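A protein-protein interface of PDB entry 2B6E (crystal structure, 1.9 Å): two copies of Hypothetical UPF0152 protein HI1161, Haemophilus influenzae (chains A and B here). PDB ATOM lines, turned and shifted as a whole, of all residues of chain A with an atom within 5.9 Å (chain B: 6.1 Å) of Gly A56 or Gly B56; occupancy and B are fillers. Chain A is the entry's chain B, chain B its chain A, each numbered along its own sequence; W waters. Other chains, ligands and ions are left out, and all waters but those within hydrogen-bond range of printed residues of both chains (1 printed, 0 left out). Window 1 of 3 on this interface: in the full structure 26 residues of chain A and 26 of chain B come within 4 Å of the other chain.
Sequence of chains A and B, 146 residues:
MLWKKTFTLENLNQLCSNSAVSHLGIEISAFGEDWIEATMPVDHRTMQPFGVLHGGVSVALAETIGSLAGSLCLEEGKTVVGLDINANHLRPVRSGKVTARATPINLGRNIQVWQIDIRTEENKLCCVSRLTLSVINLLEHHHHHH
Water W1 bridges the backbone NH (N) of Gly B55 (2.9 Å) and the side-chain carboxylate (OE2) of Glu A63 (3.2 Å).
Of the 12 printed residues of chain A, 8 touch a printed residue of chain B.
Hydrophobic or aromatic side chains of chain A that line the printed part of chain B: His A54, Val A59, Ala A60, Ile A85 and His A89.
Hydrophobic or aromatic side chains of chain B within 4 Å of the printed part of chain A: His B54, Val B59, Ala B60 and His B89.
His A54 touches Ala B60, and with the chains exchanged Ala A60 touches His B54.
Gly A55 touches Glu B63, and with the chains exchanged Glu A63 touches Gly B55.
Val A59 touches its own counterpart, Val B59.
Ile A85 touches Val B59, but with the chains exchanged Val A59 does not touch Ile B85 (4.1 Å).
11 positions are printed for both chains.
Among the printed residues, merely in contact across the chains: His A54 with Ala B60, Gly A55 with Glu B63, Gly A56 with Gly B56, Gly A56 with Ala B60, Val A59 with Val B59, Ala A60 with His B54, Ala A60 with Gly B56, Glu A63 with Gly B55 and Ile A85 with Val B59.
The side-chain carboxylate of Glu A63 is in hydrogen-bond range of the backbone NH of Gly B56 (3.4 Å).
N of Gly A56 lies within hydrogen-bond range of OE1 of Glu B63, at 3.5 Å.
The side-chain carboxylate of Glu B63 sits close to a ring nitrogen (ND1) of His A89.
The side-chain hydroxyl (OG1) of Thr B64 is in hydrogen-bond range of a ring nitrogen (NE2) of His A54, 2.8 Å away.
A ring nitrogen (ND1) of His B89 sits close to the side-chain carboxylate of Glu A63.
Gln A48 touches none of the printed residues of chain B.
Of the printed residues of chain B, Gly A56 touches Gly B56 (3.99 Å), Ala B60 (3.6 Å) and Glu B63 (3.5 Å).
Of the printed residues of chain B, Ala A60 touches His B54 and Gly B56.
Of the printed residues of chain A, Gly B55 touches Glu A63 (3.5 Å).
Printed residues of chain A within 4 Å of Gly B56: Gly A56 (3.99 Å), Ala A60 (3.6 Å) and Glu A63 (3.4 Å).
Of the printed residues of chain A, Glu B63 touches Gly A55 (3.6 Å), Gly A56 (3.5 Å) and His A89 (2.9 Å).
The nearest printed residue of chain B that does not touch Gly A56 is Val B59 (4.4 Å).
The nearest printed residue of chain B that does not touch His A89 is Ile B85 (4.1 Å).
ND1 of His B54 lies within hydrogen-bond range of N of Val B57 (3.3 Å).
OG1 of Thr B64 lies within hydrogen-bond range of O of Ala B60, at 2.9 Å.
The backbone NH of Gly A56 lies within hydrogen-bond range of a ring nitrogen (ND1) of His A54.
The backbone NH (N) of Val A57 is in hydrogen-bond range of a ring nitrogen (ND1) of His A54, 3.4 Å away.
OG of Ser A58 is in hydrogen-bond range of O of His A54 (3.5 Å).
The backbone carbonyl oxygen (O) of Gly A55 is in hydrogen-bond range of a ring nitrogen (NE2) of His A89, at 3.0 Å.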
ATOM      1  N   GLN A  48     -21.867  -8.623  -0.302  1.00  0.00           N
ATOM      2  CA  GLN A  48     -20.607  -8.589  -1.032  1.00  0.00           C
ATOM      3  C   GLN A  48     -19.591  -8.292   0.061  1.00  0.00           C
ATOM      4  O   GLN A  48     -19.965  -7.939   1.176  1.00  0.00           O
ATOM      5  CB  GLN A  48     -20.602  -7.429  -2.030  1.00  0.00           C
ATOM      6  CG  GLN A  48     -21.408  -7.642  -3.290  1.00  0.00           C
ATOM      7  CD  GLN A  48     -20.625  -8.382  -4.354  1.00  0.00           C
ATOM      8  OE1 GLN A  48     -21.049  -8.463  -5.509  1.00  0.00           O
ATOM      9  NE2 GLN A  48     -19.474  -8.929  -3.973  1.00  0.00           N
ATOM     10  N   HIS A  54     -25.252  -8.653  -2.251  1.00  0.00           N
ATOM     11  CA  HIS A  54     -24.554  -9.227  -3.401  1.00  0.00           C
ATOM     12  C   HIS A  54     -25.549  -9.394  -4.553  1.00  0.00           C
ATOM     13  O   HIS A  54     -26.530 -10.132  -4.436  1.00  0.00           O
ATOM     14  CB  HIS A  54     -23.952 -10.583  -2.998  1.00  0.00           C
ATOM     15  CG  HIS A  54     -23.068 -11.201  -4.037  1.00  0.00           C
ATOM     16  ND1 HIS A  54     -23.520 -11.544  -5.293  1.00  0.00           N
ATOM     17  CD2 HIS A  54     -21.770 -11.586  -3.987  1.00  0.00           C
ATOM     18  CE1 HIS A  54     -22.539 -12.117  -5.970  1.00  0.00           C
ATOM     19  NE2 HIS A  54     -21.467 -12.155  -5.198  1.00  0.00           N
ATOM     20  N   GLY A  55     -25.289  -8.698  -5.657  1.00  0.00           N
ATOM     21  CA  GLY A  55     -26.177  -8.755  -6.805  1.00  0.00           C
ATOM     22  C   GLY A  55     -26.456 -10.151  -7.330  1.00  0.00           C
ATOM     23  O   GLY A  55     -27.567 -10.434  -7.774  1.00  0.00           O
ATOM     24  N   GLY A  56     -25.450 -11.021  -7.291  1.00  0.00           N
ATOM     25  CA  GLY A  56     -25.635 -12.377  -7.771  1.00  0.00           C
ATOM     26  C   GLY A  56     -26.609 -13.143  -6.900  1.00  0.00           C
ATOM     27  O   GLY A  56     -27.352 -13.999  -7.385  1.00  0.00           O
ATOM     28  N   VAL A  57     -26.606 -12.834  -5.607  1.00  0.00           N
ATOM     29  CA  VAL A  57     -27.500 -13.490  -4.670  1.00  0.00           C
ATOM     30  C   VAL A  57     -28.918 -12.957  -4.849  1.00  0.00           C
ATOM     31  O   VAL A  57     -29.888 -13.665  -4.573  1.00  0.00           O
ATOM     32  CB  VAL A  57     -27.010 -13.287  -3.216  1.00  0.00           C
ATOM     33  CG1 VAL A  57     -28.030 -13.824  -2.230  1.00  0.00           C
ATOM     34  CG2 VAL A  57     -25.673 -13.994  -3.032  1.00  0.00           C
ATOM     35  N   SER A  58     -29.045 -11.715  -5.314  1.00  0.00           N
ATOM     36  CA  SER A  58     -30.371 -11.152  -5.563  1.00  0.00           C
ATOM     37  C   SER A  58     -30.982 -11.972  -6.692  1.00  0.00           C
ATOM     38  O   SER A  58     -32.169 -12.294  -6.665  1.00  0.00           O
ATOM     39  CB  SER A  58     -30.293  -9.681  -5.995  1.00  0.00           C
ATOM     40  OG  SER A  58     -29.725  -8.884  -4.981  1.00  0.00           O
ATOM     41  N   VAL A  59     -30.167 -12.322  -7.683  1.00  0.00           N
ATOM     42  CA  VAL A  59     -30.667 -13.121  -8.795  1.00  0.00           C
ATOM     43  C   VAL A  59     -31.087 -14.497  -8.287  1.00  0.00           C
ATOM     44  O   VAL A  59     -32.079 -15.060  -8.754  1.00  0.00           O
ATOM     45  CB  VAL A  59     -29.610 -13.292  -9.905  1.00  0.00           C
ATOM     46  CG1 VAL A  59     -30.197 -14.123 -11.054  1.00  0.00           C
ATOM     47  CG2 VAL A  59     -29.175 -11.924 -10.420  1.00  0.00           C
ATOM     48  N   ALA A  60     -30.335 -15.042  -7.332  1.00  0.00           N
ATOM     49  CA  ALA A  60     -30.675 -16.346  -6.759  1.00  0.00           C
ATOM     50  C   ALA A  60     -32.074 -16.267  -6.143  1.00  0.00           C
ATOM     51  O   ALA A  60     -32.894 -17.173  -6.308  1.00  0.00           O
ATOM     52  CB  ALA A  60     -29.651 -16.735  -5.693  1.00  0.00           C
ATOM     53  N   LEU A  61     -32.342 -15.181  -5.422  1.00  0.00           N
ATOM     54  CA  LEU A  61     -33.653 -14.988  -4.809  1.00  0.00           C
ATOM     55  C   LEU A  61     -34.704 -14.888  -5.915  1.00  0.00           C
ATOM     56  O   LEU A  61     -35.773 -15.503  -5.828  1.00  0.00           O
ATOM     57  CB  LEU A  61     -33.665 -13.712  -3.961  1.00  0.00           C
ATOM     58  CG  LEU A  61     -35.018 -13.177  -3.470  1.00  0.00           C
ATOM     59  CD1 LEU A  61     -35.737 -14.205  -2.591  1.00  0.00           C
ATOM     60  CD2 LEU A  61     -34.765 -11.885  -2.695  1.00  0.00           C
ATOM     61  N   GLU A  63     -34.640 -16.095  -9.035  1.00  0.00           N
ATOM     62  CA  GLU A  63     -34.893 -17.388  -9.660  1.00  0.00           C
ATOM     63  C   GLU A  63     -35.694 -18.308  -8.730  1.00  0.00           C
ATOM     64  O   GLU A  63     -36.554 -19.070  -9.180  1.00  0.00           O
ATOM     65  CB  GLU A  63     -33.580 -18.062 -10.081  1.00  0.00           C
ATOM     66  CG  GLU A  63     -33.830 -19.362 -10.838  1.00  0.00           C
ATOM     67  CD  GLU A  63     -32.798 -19.658 -11.910  1.00  0.00           C
ATOM     68  OE1 GLU A  63     -31.973 -18.780 -12.233  1.00  0.00           O
ATOM     69  OE2 GLU A  63     -32.825 -20.790 -12.440  1.00  0.00           O
ATOM     70  N   ILE A  85     -32.268 -16.455 -17.193  1.00  0.00           N
ATOM     71  CA  ILE A  85     -32.697 -15.369 -16.332  1.00  0.00           C
ATOM     72  C   ILE A  85     -31.747 -14.199 -16.529  1.00  0.00           C
ATOM     73  O   ILE A  85     -30.574 -14.388 -16.869  1.00  0.00           O
ATOM     74  CB  ILE A  85     -32.716 -15.832 -14.838  1.00  0.00           C
ATOM     75  CG1 ILE A  85     -33.267 -14.726 -13.938  1.00  0.00           C
ATOM     76  CG2 ILE A  85     -31.317 -16.243 -14.393  1.00  0.00           C
ATOM     77  CD1 ILE A  85     -33.666 -15.211 -12.560  1.00  0.00           C
ATOM     78  N   HIS A  89     -29.259  -4.524 -11.689  1.00  0.00           N
ATOM     79  CA  HIS A  89     -29.116  -4.111 -10.297  1.00  0.00           C
ATOM     80  C   HIS A  89     -29.229  -2.597 -10.334  1.00  0.00           C
ATOM     81  O   HIS A  89     -28.421  -1.920 -10.976  1.00  0.00           O
ATOM     82  CB  HIS A  89     -27.760  -4.584  -9.771  1.00  0.00           C
ATOM     83  CG  HIS A  89     -27.594  -6.070  -9.849  1.00  0.00           C
ATOM     84  ND1 HIS A  89     -26.515  -6.674 -10.461  1.00  0.00           N
ATOM     85  CD2 HIS A  89     -28.402  -7.074  -9.437  1.00  0.00           C
ATOM     86  CE1 HIS A  89     -26.670  -7.985 -10.423  1.00  0.00           C
ATOM     87  NE2 HIS A  89     -27.807  -8.255  -9.808  1.00  0.00           N
ATOM     88  N   HIS B  54     -28.671 -25.212  -7.950  1.00  0.00           N
ATOM     89  CA  HIS B  54     -29.648 -24.131  -8.065  1.00  0.00           C
ATOM     90  C   HIS B  54     -29.179 -23.119  -9.119  1.00  0.00           C
ATOM     91  O   HIS B  54     -28.122 -22.497  -8.972  1.00  0.00           O
ATOM     92  CB  HIS B  54     -29.802 -23.466  -6.690  1.00  0.00           C
ATOM     93  CG  HIS B  54     -30.911 -22.464  -6.606  1.00  0.00           C
ATOM     94  ND1 HIS B  54     -30.940 -21.317  -7.369  1.00  0.00           N
ATOM     95  CD2 HIS B  54     -32.003 -22.411  -5.806  1.00  0.00           C
ATOM     96  CE1 HIS B  54     -32.000 -20.600  -7.040  1.00  0.00           C
ATOM     97  NE2 HIS B  54     -32.662 -21.241  -6.093  1.00  0.00           N
ATOM     98  N   GLY B  55     -29.959 -22.963 -10.189  1.00  0.00           N
ATOM     99  CA  GLY B  55     -29.592 -22.036 -11.253  1.00  0.00           C
ATOM    100  C   GLY B  55     -29.303 -20.618 -10.800  1.00  0.00           C
ATOM    101  O   GLY B  55     -28.410 -19.956 -11.342  1.00  0.00           O
ATOM    102  N   GLY B  56     -30.052 -20.139  -9.813  1.00  0.00           N
ATOM    103  CA  GLY B  56     -29.824 -18.791  -9.318  1.00  0.00           C
ATOM    104  C   GLY B  56     -28.452 -18.682  -8.682  1.00  0.00           C
ATOM    105  O   GLY B  56     -27.743 -17.689  -8.864  1.00  0.00           O
ATOM    106  N   VAL B  57     -28.072 -19.711  -7.933  1.00  0.00           N
ATOM    107  CA  VAL B  57     -26.776 -19.727  -7.283  1.00  0.00           C
ATOM    108  C   VAL B  57     -25.659 -19.785  -8.326  1.00  0.00           C
ATOM    109  O   VAL B  57     -24.574 -19.239  -8.111  1.00  0.00           O
ATOM    110  CB  VAL B  57     -26.687 -20.914  -6.299  1.00  0.00           C
ATOM    111  CG1 VAL B  57     -25.305 -20.994  -5.693  1.00  0.00           C
ATOM    112  CG2 VAL B  57     -27.740 -20.731  -5.202  1.00  0.00           C
ATOM    113  N   SER B  58     -25.916 -20.425  -9.464  1.00  0.00           N
ATOM    114  CA  SER B  58     -24.903 -20.486 -10.525  1.00  0.00           C
ATOM    115  C   SER B  58     -24.648 -19.053 -11.001  1.00  0.00           C
ATOM    116  O   SER B  58     -23.513 -18.673 -11.293  1.00  0.00           O
ATOM    117  CB  SER B  58     -25.394 -21.334 -11.706  1.00  0.00           C
ATOM    118  OG  SER B  58     -25.532 -22.691 -11.325  1.00  0.00           O
ATOM    119  N   VAL B  59     -25.712 -18.263 -11.078  1.00  0.00           N
ATOM    120  CA  VAL B  59     -25.584 -16.872 -11.492  1.00  0.00           C
ATOM    121  C   VAL B  59     -24.801 -16.108 -10.417  1.00  0.00           C
ATOM    122  O   VAL B  59     -24.007 -15.226 -10.732  1.00  0.00           O
ATOM    123  CB  VAL B  59     -26.963 -16.219 -11.684  1.00  0.00           C
ATOM    124  CG1 VAL B  59     -26.804 -14.743 -12.050  1.00  0.00           C
ATOM    125  CG2 VAL B  59     -27.730 -16.954 -12.776  1.00  0.00           C
ATOM    126  N   ALA B  60     -25.031 -16.444  -9.148  1.00  0.00           N
ATOM    127  CA  ALA B  60     -24.311 -15.784  -8.055  1.00  0.00           C
ATOM    128  C   ALA B  60     -22.810 -15.990  -8.248  1.00  0.00           C
ATOM    129  O   ALA B  60     -22.021 -15.050  -8.107  1.00  0.00           O
ATOM    130  CB  ALA B  60     -24.756 -16.348  -6.707  1.00  0.00           C
ATOM    131  N   LEU B  61     -22.419 -17.226  -8.550  1.00  0.00           N
ATOM    132  CA  LEU B  61     -21.015 -17.554  -8.800  1.00  0.00           C
ATOM    133  C   LEU B  61     -20.500 -16.778 -10.012  1.00  0.00           C
ATOM    134  O   LEU B  61     -19.381 -16.254 -10.000  1.00  0.00           O
ATOM    135  CB  LEU B  61     -20.852 -19.055  -9.071  1.00  0.00           C
ATOM    136  CG  LEU B  61     -19.511 -19.530  -9.650  1.00  0.00           C
ATOM    137  CD1 LEU B  61     -18.388 -19.258  -8.646  1.00  0.00           C
ATOM    138  CD2 LEU B  61     -19.583 -21.019  -9.967  1.00  0.00           C
ATOM    139  N   GLU B  63     -21.565 -13.894 -11.276  1.00  0.00           N
ATOM    140  CA  GLU B  63     -21.359 -12.485 -10.980  1.00  0.00           C
ATOM    141  C   GLU B  63     -20.146 -12.279 -10.076  1.00  0.00           C
ATOM    142  O   GLU B  63     -19.417 -11.290 -10.215  1.00  0.00           O
ATOM    143  CB  GLU B  63     -22.597 -11.864 -10.331  1.00  0.00           C
ATOM    144  CG  GLU B  63     -22.462 -10.358 -10.223  1.00  0.00           C
ATOM    145  CD  GLU B  63     -23.787  -9.646 -10.106  1.00  0.00           C
ATOM    146  OE1 GLU B  63     -24.800 -10.179 -10.602  1.00  0.00           O
ATOM    147  OE2 GLU B  63     -23.806  -8.538  -9.534  1.00  0.00           O
ATOM    148  N   THR B  64     -19.931 -13.207  -9.150  1.00  0.00           N
ATOM    149  CA  THR B  64     -18.796 -13.106  -8.246  1.00  0.00           C
ATOM    150  C   THR B  64     -17.462 -13.098  -8.990  1.00  0.00           C
ATOM    151  O   THR B  64     -16.671 -12.162  -8.850  1.00  0.00           O
ATOM    152  CB  THR B  64     -18.771 -14.281  -7.233  1.00  0.00           C
ATOM    153  OG1 THR B  64     -19.918 -14.210  -6.372  1.00  0.00           O
ATOM    154  CG2 THR B  64     -17.506 -14.215  -6.379  1.00  0.00           C
ATOM    155  N   ILE B  85     -26.835  -8.708 -15.497  1.00  0.00           N
ATOM    156  CA  ILE B  85     -26.267 -10.001 -15.796  1.00  0.00           C
ATOM    157  C   ILE B  85     -27.363 -10.912 -16.324  1.00  0.00           C
ATOM    158  O   ILE B  85     -28.541 -10.755 -15.980  1.00  0.00           O
ATOM    159  CB  ILE B  85     -25.629 -10.604 -14.514  1.00  0.00           C
ATOM    160  CG1 ILE B  85     -24.950 -11.939 -14.825  1.00  0.00           C
ATOM    161  CG2 ILE B  85     -26.688 -10.775 -13.433  1.00  0.00           C
ATOM    162  CD1 ILE B  85     -24.076 -12.431 -13.690  1.00  0.00           C
ATOM    163  N   HIS B  89     -29.197 -21.671 -18.389  1.00  0.00           N
ATOM    164  CA  HIS B  89     -28.879 -22.902 -17.668  1.00  0.00           C
ATOM    165  C   HIS B  89     -29.023 -23.981 -18.727  1.00  0.00           C
ATOM    166  O   HIS B  89     -30.094 -24.149 -19.306  1.00  0.00           O
ATOM    167  CB  HIS B  89     -29.874 -23.073 -16.523  1.00  0.00           C
ATOM    168  CG  HIS B  89     -29.827 -21.944 -15.542  1.00  0.00           C
ATOM    169  ND1 HIS B  89     -30.957 -21.333 -15.042  1.00  0.00           N
ATOM    170  CD2 HIS B  89     -28.772 -21.275 -15.012  1.00  0.00           C
ATOM    171  CE1 HIS B  89     -30.602 -20.333 -14.254  1.00  0.00           C
ATOM    172  NE2 HIS B  89     -29.282 -20.278 -14.220  1.00  0.00           N
HETATM  173  O   HOH W   1     -32.717 -23.542 -10.796  1.00  0.00           O
